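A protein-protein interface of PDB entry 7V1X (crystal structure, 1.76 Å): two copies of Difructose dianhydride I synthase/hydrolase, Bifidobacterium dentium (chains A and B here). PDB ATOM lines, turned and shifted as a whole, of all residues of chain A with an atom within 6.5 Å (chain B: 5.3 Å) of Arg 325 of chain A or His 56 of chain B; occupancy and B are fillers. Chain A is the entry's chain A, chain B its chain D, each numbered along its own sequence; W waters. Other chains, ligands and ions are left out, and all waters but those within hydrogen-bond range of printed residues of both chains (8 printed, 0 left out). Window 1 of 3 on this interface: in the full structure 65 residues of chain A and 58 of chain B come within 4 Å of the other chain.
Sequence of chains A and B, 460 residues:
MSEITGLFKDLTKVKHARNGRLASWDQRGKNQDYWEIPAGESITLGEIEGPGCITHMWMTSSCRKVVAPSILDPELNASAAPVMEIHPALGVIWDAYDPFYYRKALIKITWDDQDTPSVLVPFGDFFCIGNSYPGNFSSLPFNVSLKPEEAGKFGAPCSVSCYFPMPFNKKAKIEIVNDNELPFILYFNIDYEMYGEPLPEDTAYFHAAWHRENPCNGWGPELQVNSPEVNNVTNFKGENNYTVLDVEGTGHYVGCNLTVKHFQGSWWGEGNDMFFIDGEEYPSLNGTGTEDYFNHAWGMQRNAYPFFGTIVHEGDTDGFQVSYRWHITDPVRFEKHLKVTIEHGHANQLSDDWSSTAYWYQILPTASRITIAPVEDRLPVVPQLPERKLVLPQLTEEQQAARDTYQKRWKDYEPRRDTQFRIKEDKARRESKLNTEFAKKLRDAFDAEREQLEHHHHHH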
ATOM      1  N   TYR A 253     -23.504 -22.801  -5.283  1.00  0.00           N
ATOM      2  CA  TYR A 253     -24.717 -23.009  -6.083  1.00  0.00           C
ATOM      3  C   TYR A 253     -24.344 -22.758  -7.543  1.00  0.00           C
ATOM      4  O   TYR A 253     -23.770 -21.715  -7.844  1.00  0.00           O
ATOM      5  CB  TYR A 253     -25.790 -22.064  -5.553  1.00  0.00           C
ATOM      6  CG  TYR A 253     -26.984 -21.814  -6.433  1.00  0.00           C
ATOM      7  CD1 TYR A 253     -28.020 -22.715  -6.503  1.00  0.00           C
ATOM      8  CD2 TYR A 253     -27.107 -20.613  -7.114  1.00  0.00           C
ATOM      9  CE1 TYR A 253     -29.168 -22.446  -7.239  1.00  0.00           C
ATOM     10  CE2 TYR A 253     -28.237 -20.326  -7.866  1.00  0.00           C
ATOM     11  CZ  TYR A 253     -29.261 -21.246  -7.933  1.00  0.00           C
ATOM     12  OH  TYR A 253     -30.354 -20.906  -8.662  1.00  0.00           O
ATOM     13  N   VAL A 254     -24.773 -23.645  -8.433  1.00  0.00           N
ATOM     14  CA  VAL A 254     -24.457 -23.527  -9.890  1.00  0.00           C
ATOM     15  C   VAL A 254     -25.744 -23.395 -10.690  1.00  0.00           C
ATOM     16  O   VAL A 254     -25.630 -23.437 -11.919  1.00  0.00           O
ATOM     17  CB  VAL A 254     -23.601 -24.714 -10.373  1.00  0.00           C
ATOM     18  CG1 VAL A 254     -22.254 -24.715  -9.687  1.00  0.00           C
ATOM     19  CG2 VAL A 254     -24.297 -26.059 -10.158  1.00  0.00           C
ATOM     20  N   GLY A 255     -26.909 -23.246 -10.043  1.00  0.00           N
ATOM     21  CA  GLY A 255     -28.116 -22.858 -10.785  1.00  0.00           C
ATOM     22  C   GLY A 255     -29.327 -23.713 -10.557  1.00  0.00           C
ATOM     23  O   GLY A 255     -29.413 -24.496  -9.570  1.00  0.00           O
ATOM     24  N   CYS A 256     -30.332 -23.481 -11.393  1.00  0.00           N
ATOM     25  CA  CYS A 256     -31.652 -24.072 -11.183  1.00  0.00           C
ATOM     26  C   CYS A 256     -32.417 -24.173 -12.488  1.00  0.00           C
ATOM     27  O   CYS A 256     -32.086 -23.483 -13.466  1.00  0.00           O
ATOM     28  CB  CYS A 256     -32.441 -23.304 -10.139  1.00  0.00           C
ATOM     29  SG  CYS A 256     -33.088 -21.708 -10.733  1.00  0.00           S
ATOM     30  N   ASN A 257     -33.406 -25.022 -12.461  1.00  0.00           N
ATOM     31  CA  ASN A 257     -34.570 -24.886 -13.367  1.00  0.00           C
ATOM     32  C   ASN A 257     -35.766 -24.522 -12.501  1.00  0.00           C
ATOM     33  O   ASN A 257     -35.757 -24.792 -11.287  1.00  0.00           O
ATOM     34  CB  ASN A 257     -34.723 -26.090 -14.301  1.00  0.00           C
ATOM     35  CG  ASN A 257     -34.939 -27.398 -13.577  1.00  0.00           C
ATOM     36  OD1 ASN A 257     -35.864 -27.510 -12.766  1.00  0.00           O
ATOM     37  ND2 ASN A 257     -34.098 -28.374 -13.883  1.00  0.00           N
ATOM     38  N   ASP A 273     -34.954 -12.337  -7.182  1.00  0.00           N
ATOM     39  CA  ASP A 273     -34.034 -13.292  -6.519  1.00  0.00           C
ATOM     40  C   ASP A 273     -33.390 -12.586  -5.334  1.00  0.00           C
ATOM     41  O   ASP A 273     -33.084 -11.396  -5.479  1.00  0.00           O
ATOM     42  CB  ASP A 273     -32.906 -13.789  -7.409  1.00  0.00           C
ATOM     43  CG  ASP A 273     -32.202 -12.727  -8.245  1.00  0.00           C
ATOM     44  OD1 ASP A 273     -32.903 -11.936  -8.962  1.00  0.00           O
ATOM     45  OD2 ASP A 273     -30.956 -12.697  -8.146  1.00  0.00           O
ATOM     46  N   ASP A 292     -35.417 -11.410 -14.993  1.00  0.00           N
ATOM     47  CA  ASP A 292     -34.093 -10.762 -14.898  1.00  0.00           C
ATOM     48  C   ASP A 292     -33.093 -11.759 -14.334  1.00  0.00           C
ATOM     49  O   ASP A 292     -31.945 -11.783 -14.836  1.00  0.00           O
ATOM     50  CB  ASP A 292     -34.137  -9.519 -14.034  1.00  0.00           C
ATOM     51  CG  ASP A 292     -35.212  -8.543 -14.450  1.00  0.00           C
ATOM     52  OD1 ASP A 292     -35.842  -8.758 -15.555  1.00  0.00           O
ATOM     53  OD2 ASP A 292     -35.440  -7.606 -13.650  1.00  0.00           O
ATOM     54  N   TYR A 293     -33.484 -12.511 -13.305  1.00  0.00           N
ATOM     55  CA  TYR A 293     -32.616 -13.599 -12.764  1.00  0.00           C
ATOM     56  C   TYR A 293     -32.252 -14.565 -13.896  1.00  0.00           C
ATOM     57  O   TYR A 293     -31.052 -14.945 -14.000  1.00  0.00           O
ATOM     58  CB  TYR A 293     -33.264 -14.320 -11.582  1.00  0.00           C
ATOM     59  CG  TYR A 293     -32.433 -15.490 -11.150  1.00  0.00           C
ATOM     60  CD1 TYR A 293     -31.233 -15.305 -10.476  1.00  0.00           C
ATOM     61  CD2 TYR A 293     -32.848 -16.781 -11.416  1.00  0.00           C
ATOM     62  CE1 TYR A 293     -30.421 -16.379 -10.157  1.00  0.00           C
ATOM     63  CE2 TYR A 293     -32.058 -17.863 -11.094  1.00  0.00           C
ATOM     64  CZ  TYR A 293     -30.855 -17.665 -10.432  1.00  0.00           C
ATOM     65  OH  TYR A 293     -30.021 -18.710 -10.163  1.00  0.00           O
ATOM     66  N   PHE A 294     -33.224 -14.971 -14.741  1.00  0.00           N
ATOM     67  CA  PHE A 294     -32.958 -15.843 -15.915  1.00  0.00           C
ATOM     68  C   PHE A 294     -32.295 -15.094 -17.069  1.00  0.00           C
ATOM     69  O   PHE A 294     -32.064 -15.769 -18.095  1.00  0.00           O
ATOM     70  CB  PHE A 294     -34.213 -16.615 -16.336  1.00  0.00           C
ATOM     71  CG  PHE A 294     -34.638 -17.562 -15.240  1.00  0.00           C
ATOM     72  CD1 PHE A 294     -33.838 -18.655 -14.899  1.00  0.00           C
ATOM     73  CD2 PHE A 294     -35.836 -17.397 -14.575  1.00  0.00           C
ATOM     74  CE1 PHE A 294     -34.202 -19.489 -13.854  1.00  0.00           C
ATOM     75  CE2 PHE A 294     -36.184 -18.191 -13.501  1.00  0.00           C
ATOM     76  CZ  PHE A 294     -35.388 -19.266 -13.160  1.00  0.00           C
ATOM     77  N   ASN A 295     -31.859 -13.831 -16.872  1.00  0.00           N
ATOM     78  CA  ASN A 295     -31.092 -13.031 -17.857  1.00  0.00           C
ATOM     79  C   ASN A 295     -31.918 -12.817 -19.136  1.00  0.00           C
ATOM     80  O   ASN A 295     -31.343 -12.525 -20.140  1.00  0.00           O
ATOM     81  CB  ASN A 295     -29.719 -13.630 -18.158  1.00  0.00           C
ATOM     82  CG  ASN A 295     -28.704 -13.251 -17.099  1.00  0.00           C
ATOM     83  OD1 ASN A 295     -27.648 -12.725 -17.422  1.00  0.00           O
ATOM     84  ND2 ASN A 295     -29.059 -13.498 -15.858  1.00  0.00           N
ATOM     85  N   PHE A 307     -25.919 -20.352 -20.680  1.00  0.00           N
ATOM     86  CA  PHE A 307     -25.999 -20.177 -19.203  1.00  0.00           C
ATOM     87  C   PHE A 307     -27.414 -19.855 -18.717  1.00  0.00           C
ATOM     88  O   PHE A 307     -27.621 -19.757 -17.504  1.00  0.00           O
ATOM     89  CB  PHE A 307     -24.983 -19.149 -18.708  1.00  0.00           C
ATOM     90  CG  PHE A 307     -23.559 -19.456 -19.068  1.00  0.00           C
ATOM     91  CD1 PHE A 307     -22.958 -20.648 -18.699  1.00  0.00           C
ATOM     92  CD2 PHE A 307     -22.789 -18.509 -19.711  1.00  0.00           C
ATOM     93  CE1 PHE A 307     -21.623 -20.899 -18.991  1.00  0.00           C
ATOM     94  CE2 PHE A 307     -21.464 -18.762 -20.022  1.00  0.00           C
ATOM     95  CZ  PHE A 307     -20.887 -19.971 -19.683  1.00  0.00           C
ATOM     96  N   PHE A 308     -28.388 -19.741 -19.593  1.00  0.00           N
ATOM     97  CA  PHE A 308     -29.741 -19.334 -19.143  1.00  0.00           C
ATOM     98  C   PHE A 308     -30.746 -19.422 -20.283  1.00  0.00           C
ATOM     99  O   PHE A 308     -30.370 -19.206 -21.447  1.00  0.00           O
ATOM    100  CB  PHE A 308     -29.719 -17.916 -18.557  1.00  0.00           C
ATOM    101  CG  PHE A 308     -29.231 -16.857 -19.499  1.00  0.00           C
ATOM    102  CD1 PHE A 308     -30.087 -16.311 -20.466  1.00  0.00           C
ATOM    103  CD2 PHE A 308     -27.907 -16.422 -19.463  1.00  0.00           C
ATOM    104  CE1 PHE A 308     -29.654 -15.325 -21.319  1.00  0.00           C
ATOM    105  CE2 PHE A 308     -27.481 -15.436 -20.335  1.00  0.00           C
ATOM    106  CZ  PHE A 308     -28.354 -14.889 -21.255  1.00  0.00           C
ATOM    107  N   GLY A 309     -32.009 -19.535 -19.912  1.00  0.00           N
ATOM    108  CA  GLY A 309     -33.087 -19.253 -20.854  1.00  0.00           C
ATOM    109  C   GLY A 309     -34.332 -20.047 -20.572  1.00  0.00           C
ATOM    110  O   GLY A 309     -34.634 -20.366 -19.398  1.00  0.00           O
ATOM    111  N   SER A 323     -37.852 -22.542 -17.048  1.00  0.00           N
ATOM    112  CA  SER A 323     -36.672 -21.689 -17.306  1.00  0.00           C
ATOM    113  C   SER A 323     -35.444 -22.308 -16.602  1.00  0.00           C
ATOM    114  O   SER A 323     -35.601 -23.179 -15.730  1.00  0.00           O
ATOM    115  CB  SER A 323     -36.903 -20.254 -16.868  1.00  0.00           C
ATOM    116  OG  SER A 323     -38.203 -19.788 -17.240  1.00  0.00           O
ATOM    117  N   TYR A 324     -34.256 -21.821 -16.894  1.00  0.00           N
ATOM    118  CA  TYR A 324     -33.008 -22.275 -16.226  1.00  0.00           C
ATOM    119  C   TYR A 324     -31.981 -21.160 -16.219  1.00  0.00           C
ATOM    120  O   TYR A 324     -31.934 -20.275 -17.083  1.00  0.00           O
ATOM    121  CB  TYR A 324     -32.380 -23.476 -16.934  1.00  0.00           C
ATOM    122  CG  TYR A 324     -31.875 -23.199 -18.330  1.00  0.00           C
ATOM    123  CD1 TYR A 324     -32.758 -23.183 -19.395  1.00  0.00           C
ATOM    124  CD2 TYR A 324     -30.545 -22.955 -18.600  1.00  0.00           C
ATOM    125  CE1 TYR A 324     -32.354 -22.875 -20.681  1.00  0.00           C
ATOM    126  CE2 TYR A 324     -30.106 -22.702 -19.895  1.00  0.00           C
ATOM    127  CZ  TYR A 324     -31.015 -22.668 -20.940  1.00  0.00           C
ATOM    128  OH  TYR A 324     -30.559 -22.433 -22.198  1.00  0.00           O
ATOM    129  N   ARG A 325     -31.098 -21.240 -15.245  1.00  0.00           N
ATOM    130  CA  ARG A 325     -29.860 -20.439 -15.219  1.00  0.00           C
ATOM    131  C   ARG A 325     -28.760 -21.303 -14.617  1.00  0.00           C
ATOM    132  O   ARG A 325     -29.033 -21.958 -13.586  1.00  0.00           O
ATOM    133  CB  ARG A 325     -30.033 -19.164 -14.410  1.00  0.00           C
ATOM    134  CG  ARG A 325     -28.716 -18.441 -14.266  1.00  0.00           C
ATOM    135  CD  ARG A 325     -28.863 -16.987 -14.152  1.00  0.00           C
ATOM    136  NE  ARG A 325     -27.592 -16.389 -13.853  1.00  0.00           N
ATOM    137  CZ  ARG A 325     -27.472 -15.246 -13.187  1.00  0.00           C
ATOM    138  NH1 ARG A 325     -28.573 -14.619 -12.774  1.00  0.00           N
ATOM    139  NH2 ARG A 325     -26.262 -14.763 -12.921  1.00  0.00           N
ATOM    140  N   TRP A 326     -27.594 -21.276 -15.244  1.00  0.00           N
ATOM    141  CA  TRP A 326     -26.367 -21.949 -14.761  1.00  0.00           C
ATOM    142  C   TRP A 326     -25.387 -20.863 -14.337  1.00  0.00           C
ATOM    143  O   TRP A 326     -25.146 -19.921 -15.096  1.00  0.00           O
ATOM    144  CB  TRP A 326     -25.744 -22.884 -15.788  1.00  0.00           C
ATOM    145  CG  TRP A 326     -26.742 -23.791 -16.435  1.00  0.00           C
ATOM    146  CD1 TRP A 326     -27.004 -23.924 -17.761  1.00  0.00           C
ATOM    147  CD2 TRP A 326     -27.620 -24.696 -15.752  1.00  0.00           C
ATOM    148  NE1 TRP A 326     -27.989 -24.848 -17.953  1.00  0.00           N
ATOM    149  CE2 TRP A 326     -28.401 -25.324 -16.740  1.00  0.00           C
ATOM    150  CE3 TRP A 326     -27.822 -25.030 -14.404  1.00  0.00           C
ATOM    151  CZ2 TRP A 326     -29.353 -26.275 -16.423  1.00  0.00           C
ATOM    152  CZ3 TRP A 326     -28.757 -25.993 -14.086  1.00  0.00           C
ATOM    153  CH2 TRP A 326     -29.537 -26.575 -15.094  1.00  0.00           C
ATOM    154  N   HIS A 327     -24.890 -21.000 -13.126  1.00  0.00           N
ATOM    155  CA  HIS A 327     -23.814 -20.167 -12.565  1.00  0.00           C
ATOM    156  C   HIS A 327     -22.541 -20.994 -12.621  1.00  0.00           C
ATOM    157  O   HIS A 327     -22.181 -21.558 -11.586  1.00  0.00           O
ATOM    158  CB  HIS A 327     -24.167 -19.730 -11.147  1.00  0.00           C
ATOM    159  CG  HIS A 327     -25.413 -18.941 -10.997  1.00  0.00           C
ATOM    160  ND1 HIS A 327     -25.408 -17.578 -10.725  1.00  0.00           N
ATOM    161  CD2 HIS A 327     -26.709 -19.320 -10.948  1.00  0.00           C
ATOM    162  CE1 HIS A 327     -26.652 -17.164 -10.572  1.00  0.00           C
ATOM    163  NE2 HIS A 327     -27.463 -18.190 -10.688  1.00  0.00           N
ATOM    164  N   THR A 329     -19.386 -20.005 -14.465  1.00  0.00           N
ATOM    165  CA  THR A 329     -18.238 -19.090 -14.277  1.00  0.00           C
ATOM    166  C   THR A 329     -18.553 -18.081 -13.155  1.00  0.00           C
ATOM    167  O   THR A 329     -17.624 -17.404 -12.725  1.00  0.00           O
ATOM    168  CB  THR A 329     -17.867 -18.462 -15.623  1.00  0.00           C
ATOM    169  OG1 THR A 329     -18.900 -17.542 -15.972  1.00  0.00           O
ATOM    170  CG2 THR A 329     -17.689 -19.488 -16.718  1.00  0.00           C
ATOM    171  N   ASP A 330     -19.823 -17.957 -12.722  1.00  0.00           N
ATOM    172  CA  ASP A 330     -20.315 -16.962 -11.727  1.00  0.00           C
ATOM    173  C   ASP A 330     -21.069 -17.677 -10.611  1.00  0.00           C
ATOM    174  O   ASP A 330     -22.177 -17.259 -10.216  1.00  0.00           O
ATOM    175  CB  ASP A 330     -21.237 -15.906 -12.348  1.00  0.00           C
ATOM    176  CG  ASP A 330     -22.420 -16.486 -13.115  1.00  0.00           C
ATOM    177  OD1 ASP A 330     -22.293 -17.636 -13.618  1.00  0.00           O
ATOM    178  OD2 ASP A 330     -23.451 -15.795 -13.180  1.00  0.00           O
ATOM    179  N   TYR A 359     -29.190 -26.992  -8.085  1.00  0.00           N
ATOM    180  CA  TYR A 359     -27.942 -27.746  -8.327  1.00  0.00           C
ATOM    181  C   TYR A 359     -26.804 -27.052  -7.609  1.00  0.00           C
ATOM    182  O   TYR A 359     -26.685 -25.809  -7.695  1.00  0.00           O
ATOM    183  CB  TYR A 359     -27.607 -27.801  -9.810  1.00  0.00           C
ATOM    184  CG  TYR A 359     -28.681 -28.420 -10.674  1.00  0.00           C
ATOM    185  CD1 TYR A 359     -29.736 -27.640 -11.107  1.00  0.00           C
ATOM    186  CD2 TYR A 359     -28.675 -29.737 -11.059  1.00  0.00           C
ATOM    187  CE1 TYR A 359     -30.731 -28.150 -11.929  1.00  0.00           C
ATOM    188  CE2 TYR A 359     -29.656 -30.272 -11.891  1.00  0.00           C
ATOM    189  CZ  TYR A 359     -30.675 -29.460 -12.363  1.00  0.00           C
ATOM    190  OH  TYR A 359     -31.689 -29.934 -13.168  1.00  0.00           O
ATOM    191  N   ILE B  54     -15.217  -9.055 -11.303  1.00  0.00           N
ATOM    192  CA  ILE B  54     -16.552  -9.088 -11.954  1.00  0.00           C
ATOM    193  C   ILE B  54     -16.656 -10.443 -12.665  1.00  0.00           C
ATOM    194  O   ILE B  54     -15.793 -10.751 -13.476  1.00  0.00           O
ATOM    195  CB  ILE B  54     -16.742  -7.914 -12.927  1.00  0.00           C
ATOM    196  CG1 ILE B  54     -16.350  -6.569 -12.300  1.00  0.00           C
ATOM    197  CG2 ILE B  54     -18.166  -7.887 -13.445  1.00  0.00           C
ATOM    198  CD1 ILE B  54     -17.192  -6.174 -11.131  1.00  0.00           C
ATOM    199  N   THR B  55     -17.747 -11.156 -12.431  1.00  0.00           N
ATOM    200  CA  THR B  55     -18.021 -12.470 -13.047  1.00  0.00           C
ATOM    201  C   THR B  55     -19.191 -12.425 -14.029  1.00  0.00           C
ATOM    202  O   THR B  55     -19.288 -13.340 -14.862  1.00  0.00           O
ATOM    203  CB  THR B  55     -18.354 -13.498 -11.968  1.00  0.00           C
ATOM    204  OG1 THR B  55     -19.487 -13.072 -11.227  1.00  0.00           O
ATOM    205  CG2 THR B  55     -17.155 -13.749 -11.081  1.00  0.00           C
ATOM    206  N   HIS B  56     -20.096 -11.467 -13.925  1.00  0.00           N
ATOM    207  CA  HIS B  56     -21.329 -11.484 -14.742  1.00  0.00           C
ATOM    208  C   HIS B  56     -22.002 -10.129 -14.676  1.00  0.00           C
ATOM    209  O   HIS B  56     -22.125  -9.556 -13.577  1.00  0.00           O
ATOM    210  CB  HIS B  56     -22.265 -12.585 -14.241  1.00  0.00           C
ATOM    211  CG  HIS B  56     -23.686 -12.446 -14.647  1.00  0.00           C
ATOM    212  ND1 HIS B  56     -24.630 -11.847 -13.822  1.00  0.00           N
ATOM    213  CD2 HIS B  56     -24.297 -12.739 -15.825  1.00  0.00           C
ATOM    214  CE1 HIS B  56     -25.797 -11.872 -14.447  1.00  0.00           C
ATOM    215  NE2 HIS B  56     -25.621 -12.431 -15.688  1.00  0.00           N
ATOM    216  N   MET B  57     -22.442  -9.641 -15.821  1.00  0.00           N
ATOM    217  CA  MET B  57     -23.323  -8.462 -15.882  1.00  0.00           C
ATOM    218  C   MET B  57     -24.555  -8.829 -16.697  1.00  0.00           C
ATOM    219  O   MET B  57     -24.410  -9.532 -17.734  1.00  0.00           O
ATOM    220  CB  MET B  57     -22.609  -7.294 -16.544  1.00  0.00           C
ATOM    221  CG  MET B  57     -21.330  -6.933 -15.892  1.00  0.00           C
ATOM    222  SD  MET B  57     -20.847  -5.279 -16.537  1.00  0.00           S
ATOM    223  CE  MET B  57     -19.294  -5.037 -15.699  1.00  0.00           C
ATOM    224  N   TRP B  58     -25.704  -8.421 -16.196  1.00  0.00           N
ATOM    225  CA  TRP B  58     -26.980  -8.447 -16.933  1.00  0.00           C
ATOM    226  C   TRP B  58     -27.586  -7.044 -16.809  1.00  0.00           C
ATOM    227  O   TRP B  58     -27.551  -6.453 -15.707  1.00  0.00           O
ATOM    228  CB  TRP B  58     -27.905  -9.485 -16.342  1.00  0.00           C
ATOM    229  CG  TRP B  58     -29.298  -9.269 -16.813  1.00  0.00           C
ATOM    230  CD1 TRP B  58     -29.841  -9.846 -17.930  1.00  0.00           C
ATOM    231  CD2 TRP B  58     -30.315  -8.415 -16.248  1.00  0.00           C
ATOM    232  NE1 TRP B  58     -31.130  -9.424 -18.086  1.00  0.00           N
ATOM    233  CE2 TRP B  58     -31.459  -8.558 -17.074  1.00  0.00           C
ATOM    234  CE3 TRP B  58     -30.414  -7.622 -15.095  1.00  0.00           C
ATOM    235  CZ2 TRP B  58     -32.664  -7.912 -16.805  1.00  0.00           C
ATOM    236  CZ3 TRP B  58     -31.591  -6.936 -14.854  1.00  0.00           C
ATOM    237  CH2 TRP B  58     -32.697  -7.088 -15.690  1.00  0.00           C
ATOM    238  N   SER B 161     -26.162  -9.489 -21.590  1.00  0.00           N
ATOM    239  CA  SER B 161     -25.377 -10.202 -20.571  1.00  0.00           C
ATOM    240  C   SER B 161     -23.939 -10.327 -21.056  1.00  0.00           C
ATOM    241  O   SER B 161     -23.674 -10.523 -22.257  1.00  0.00           O
ATOM    242  CB  SER B 161     -25.988 -11.523 -20.210  1.00  0.00           C
ATOM    243  OG  SER B 161     -26.282 -12.251 -21.374  1.00  0.00           O
ATOM    244  N   CYS B 162     -23.037 -10.160 -20.112  1.00  0.00           N
ATOM    245  CA  CYS B 162     -21.594 -10.212 -20.321  1.00  0.00           C
ATOM    246  C   CYS B 162     -20.967 -11.179 -19.307  1.00  0.00           C
ATOM    247  O   CYS B 162     -21.211 -11.031 -18.110  1.00  0.00           O
ATOM    248  CB  CYS B 162     -20.991  -8.832 -20.184  1.00  0.00           C
ATOM    249  SG  CYS B 162     -19.200  -8.902 -20.396  1.00  0.00           S
ATOM    250  N   TYR B 163     -20.220 -12.161 -19.769  1.00  0.00           N
ATOM    251  CA  TYR B 163     -19.513 -13.157 -18.932  1.00  0.00           C
ATOM    252  C   TYR B 163     -17.994 -13.014 -19.007  1.00  0.00           C
ATOM    253  O   TYR B 163     -17.292 -13.885 -18.446  1.00  0.00           O
ATOM    254  CB  TYR B 163     -19.942 -14.572 -19.323  1.00  0.00           C
ATOM    255  CG  TYR B 163     -21.302 -14.931 -18.802  1.00  0.00           C
ATOM    256  CD1 TYR B 163     -21.458 -15.467 -17.542  1.00  0.00           C
ATOM    257  CD2 TYR B 163     -22.440 -14.647 -19.555  1.00  0.00           C
ATOM    258  CE1 TYR B 163     -22.713 -15.808 -17.068  1.00  0.00           C
ATOM    259  CE2 TYR B 163     -23.700 -14.990 -19.093  1.00  0.00           C
ATOM    260  CZ  TYR B 163     -23.836 -15.554 -17.832  1.00  0.00           C
ATOM    261  OH  TYR B 163     -25.065 -15.872 -17.358  1.00  0.00           O
ATOM    262  N   ASN B 189     -27.843  -6.126 -12.897  1.00  0.00           N
ATOM    263  CA  ASN B 189     -27.269  -7.033 -11.872  1.00  0.00           C
ATOM    264  C   ASN B 189     -25.826  -7.240 -12.297  1.00  0.00           C
ATOM    265  O   ASN B 189     -25.615  -7.814 -13.378  1.00  0.00           O
ATOM    266  CB  ASN B 189     -27.926  -8.425 -11.764  1.00  0.00           C
ATOM    267  CG  ASN B 189     -29.432  -8.527 -11.688  1.00  0.00           C
ATOM    268  OD1 ASN B 189     -30.002  -9.612 -11.919  1.00  0.00           O
ATOM    269  ND2 ASN B 189     -30.135  -7.452 -11.403  1.00  0.00           N
ATOM    270  N   ILE B 190     -24.870  -6.805 -11.481  1.00  0.00           N
ATOM    271  CA  ILE B 190     -23.409  -6.933 -11.709  1.00  0.00           C
ATOM    272  C   ILE B 190     -22.847  -7.765 -10.566  1.00  0.00           C
ATOM    273  O   ILE B 190     -22.816  -7.284  -9.424  1.00  0.00           O
ATOM    274  CB  ILE B 190     -22.753  -5.542 -11.773  1.00  0.00           C
ATOM    275  CG1 ILE B 190     -23.318  -4.706 -12.924  1.00  0.00           C
ATOM    276  CG2 ILE B 190     -21.238  -5.653 -11.882  1.00  0.00           C
ATOM    277  CD1 ILE B 190     -22.824  -3.272 -12.889  1.00  0.00           C
ATOM    278  N   ASP B 191     -22.488  -8.991 -10.871  1.00  0.00           N
ATOM    279  CA  ASP B 191     -22.072 -10.020  -9.903  1.00  0.00           C
ATOM    280  C   ASP B 191     -20.552 -10.027  -9.869  1.00  0.00           C
ATOM    281  O   ASP B 191     -19.918  -9.887 -10.922  1.00  0.00           O
ATOM    282  CB  ASP B 191     -22.666 -11.371 -10.279  1.00  0.00           C
ATOM    283  CG  ASP B 191     -24.176 -11.417 -10.059  1.00  0.00           C
ATOM    284  OD1 ASP B 191     -24.609 -11.540  -8.872  1.00  0.00           O
ATOM    285  OD2 ASP B 191     -24.912 -11.294 -11.067  1.00  0.00           O
HETATM  286  O   HOH W   1     -17.746 -15.110 -16.127  1.00  0.00           O
HETATM  287  O   HOH W   2     -27.012 -12.662 -10.887  1.00  0.00           O
HETATM  288  O   HOH W   3     -32.702 -10.347 -10.966  1.00  0.00           O
HETATM  289  O   HOH W   4     -25.053 -17.323 -15.016  1.00  0.00           O
HETATM  290  O   HOH W   5     -29.512 -11.997 -10.462  1.00  0.00           O
HETATM  291  O   HOH W   6     -29.156 -11.433 -13.723  1.00  0.00           O
HETATM  292  O   HOH W   7     -24.012 -14.213 -11.336  1.00  0.00           O
HETATM  293  O   HOH W   8     -28.814 -11.623 -22.288  1.00  0.00           O
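A ring nitrogen (NE2) of His 56 of chain B lies within hydrogen-bond range of the side-chain amide oxygen (OD1) of Asn 295 of chain A (2.7 Å).
The guanidinium group (NH2) of Arg 325 of chain A sits close to a ring nitrogen (ND1) of His 56 of chain B (3.5 Å).
The backbone NH (N) of Cys 256 of chain A lies within hydrogen-bond range of the backbone carbonyl oxygen (O) of Arg 325 of chain A (3.0 Å).
The backbone carbonyl oxygen of Tyr 293 of chain A sits at hydrogen-bond distance from the side-chain amide nitrogen of Asn 295 of chain A, 3.1 Å away.
O of Phe 307 of chain A lies within hydrogen-bond range of N of Trp 326 of chain A, at 2.7 Å.
The side-chain hydroxyl (OH) of Tyr 324 of chain A is in hydrogen-bond range of the backbone carbonyl oxygen (O) of Phe 308 of chain A, 3.3 Å away.
The backbone carbonyl oxygen (O) of Asp 191 of chain B lies within hydrogen-bond range of the backbone NH (N) of Thr 55 of chain B (2.9 Å).
Among the printed residues, pairs that only touch across the chains: Asp 292 of chain A with Trp 58 of chain B, Asn 295 of chain A with Trp 58 of chain B, Asn 295 of chain A with Ser 161 of chain B, Phe 307 of chain A with Tyr 163 of chain B, Phe 308 of chain A with Ser 161 of chain B, Phe 308 of chain A with Tyr 163 of chain B, Thr 329 of chain A with Tyr 163 of chain B, Asp 330 of chain A with Thr 55 of chain B, Asp 330 of chain A with His 56 of chain B and Asp 330 of chain A with Tyr 163 of chain B.
Of the printed residues of chain B, Asp 292 of chain A touches Trp 58 (3.2 Å).
Trp 326 of chain A touches none of the printed residues of chain B.
Of the printed residues of chain B, Asp 330 of chain A touches Thr 55, His 56 and Tyr 163.
Of the printed residues of chain A, Thr 55 of chain B touches Asp 330.
Of chain A, only Asn 295 (2.7 Å), Arg 325 (3.3 Å) and Asp 330 (3.6 Å) come within 4 Å of His 56 of chain B.
Of the printed residues of chain A, Tyr 163 of chain B touches Phe 307 (3.5 Å), Phe 308 (3.6 Å), Thr 329 (3.6 Å) and Asp 330 (3.9 Å).
The nearest residue of chain B that does not touch Arg 325 of chain A is Asp 191 of chain B (4.2 Å).
The nearest residue of chain A that does not touch His 56 of chain B is Phe 308 of chain A (5.8 Å).
The nearest printed residue of chain B that does not touch Asn 295 of chain A is Tyr 163 of chain B (4.1 Å).
Hydrophobic or aromatic side chains of chain B within 4 Å of the printed part of chain A: His 56, Trp 58 and Tyr 163.
Among the printed residues, no Asp or Glu carboxylate lies within 4 Å of a Lys or Arg side-chain nitrogen of the other chain.
No position is printed for both chains.
Water W3 lies within hydrogen-bond range of OD1 of Asp 273 of chain A (2.6 Å), OD1 of Asn 189 of chain B (3.0 Å) and N of Tyr 293 of chain A (3.3 Å).
Water W1 lies within hydrogen-bond range of the backbone carbonyl oxygen of Tyr 163 of chain B (2.7 Å), the backbone carbonyl oxygen of Thr 55 of chain B (2.7 Å) and the side-chain hydroxyl of Thr 329 of chain A (2.7 Å).
Water W8 bridges the side-chain hydroxyl of Ser 161 of chain B (2.8 Å) and the backbone carbonyl oxygen of Asn 295 of chain A (3.4 Å).
Water W5 lies within hydrogen-bond range of OD2 of Asp 273 of chain A (2.8 Å) and OD1 of Asn 189 of chain B (2.8 Å).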
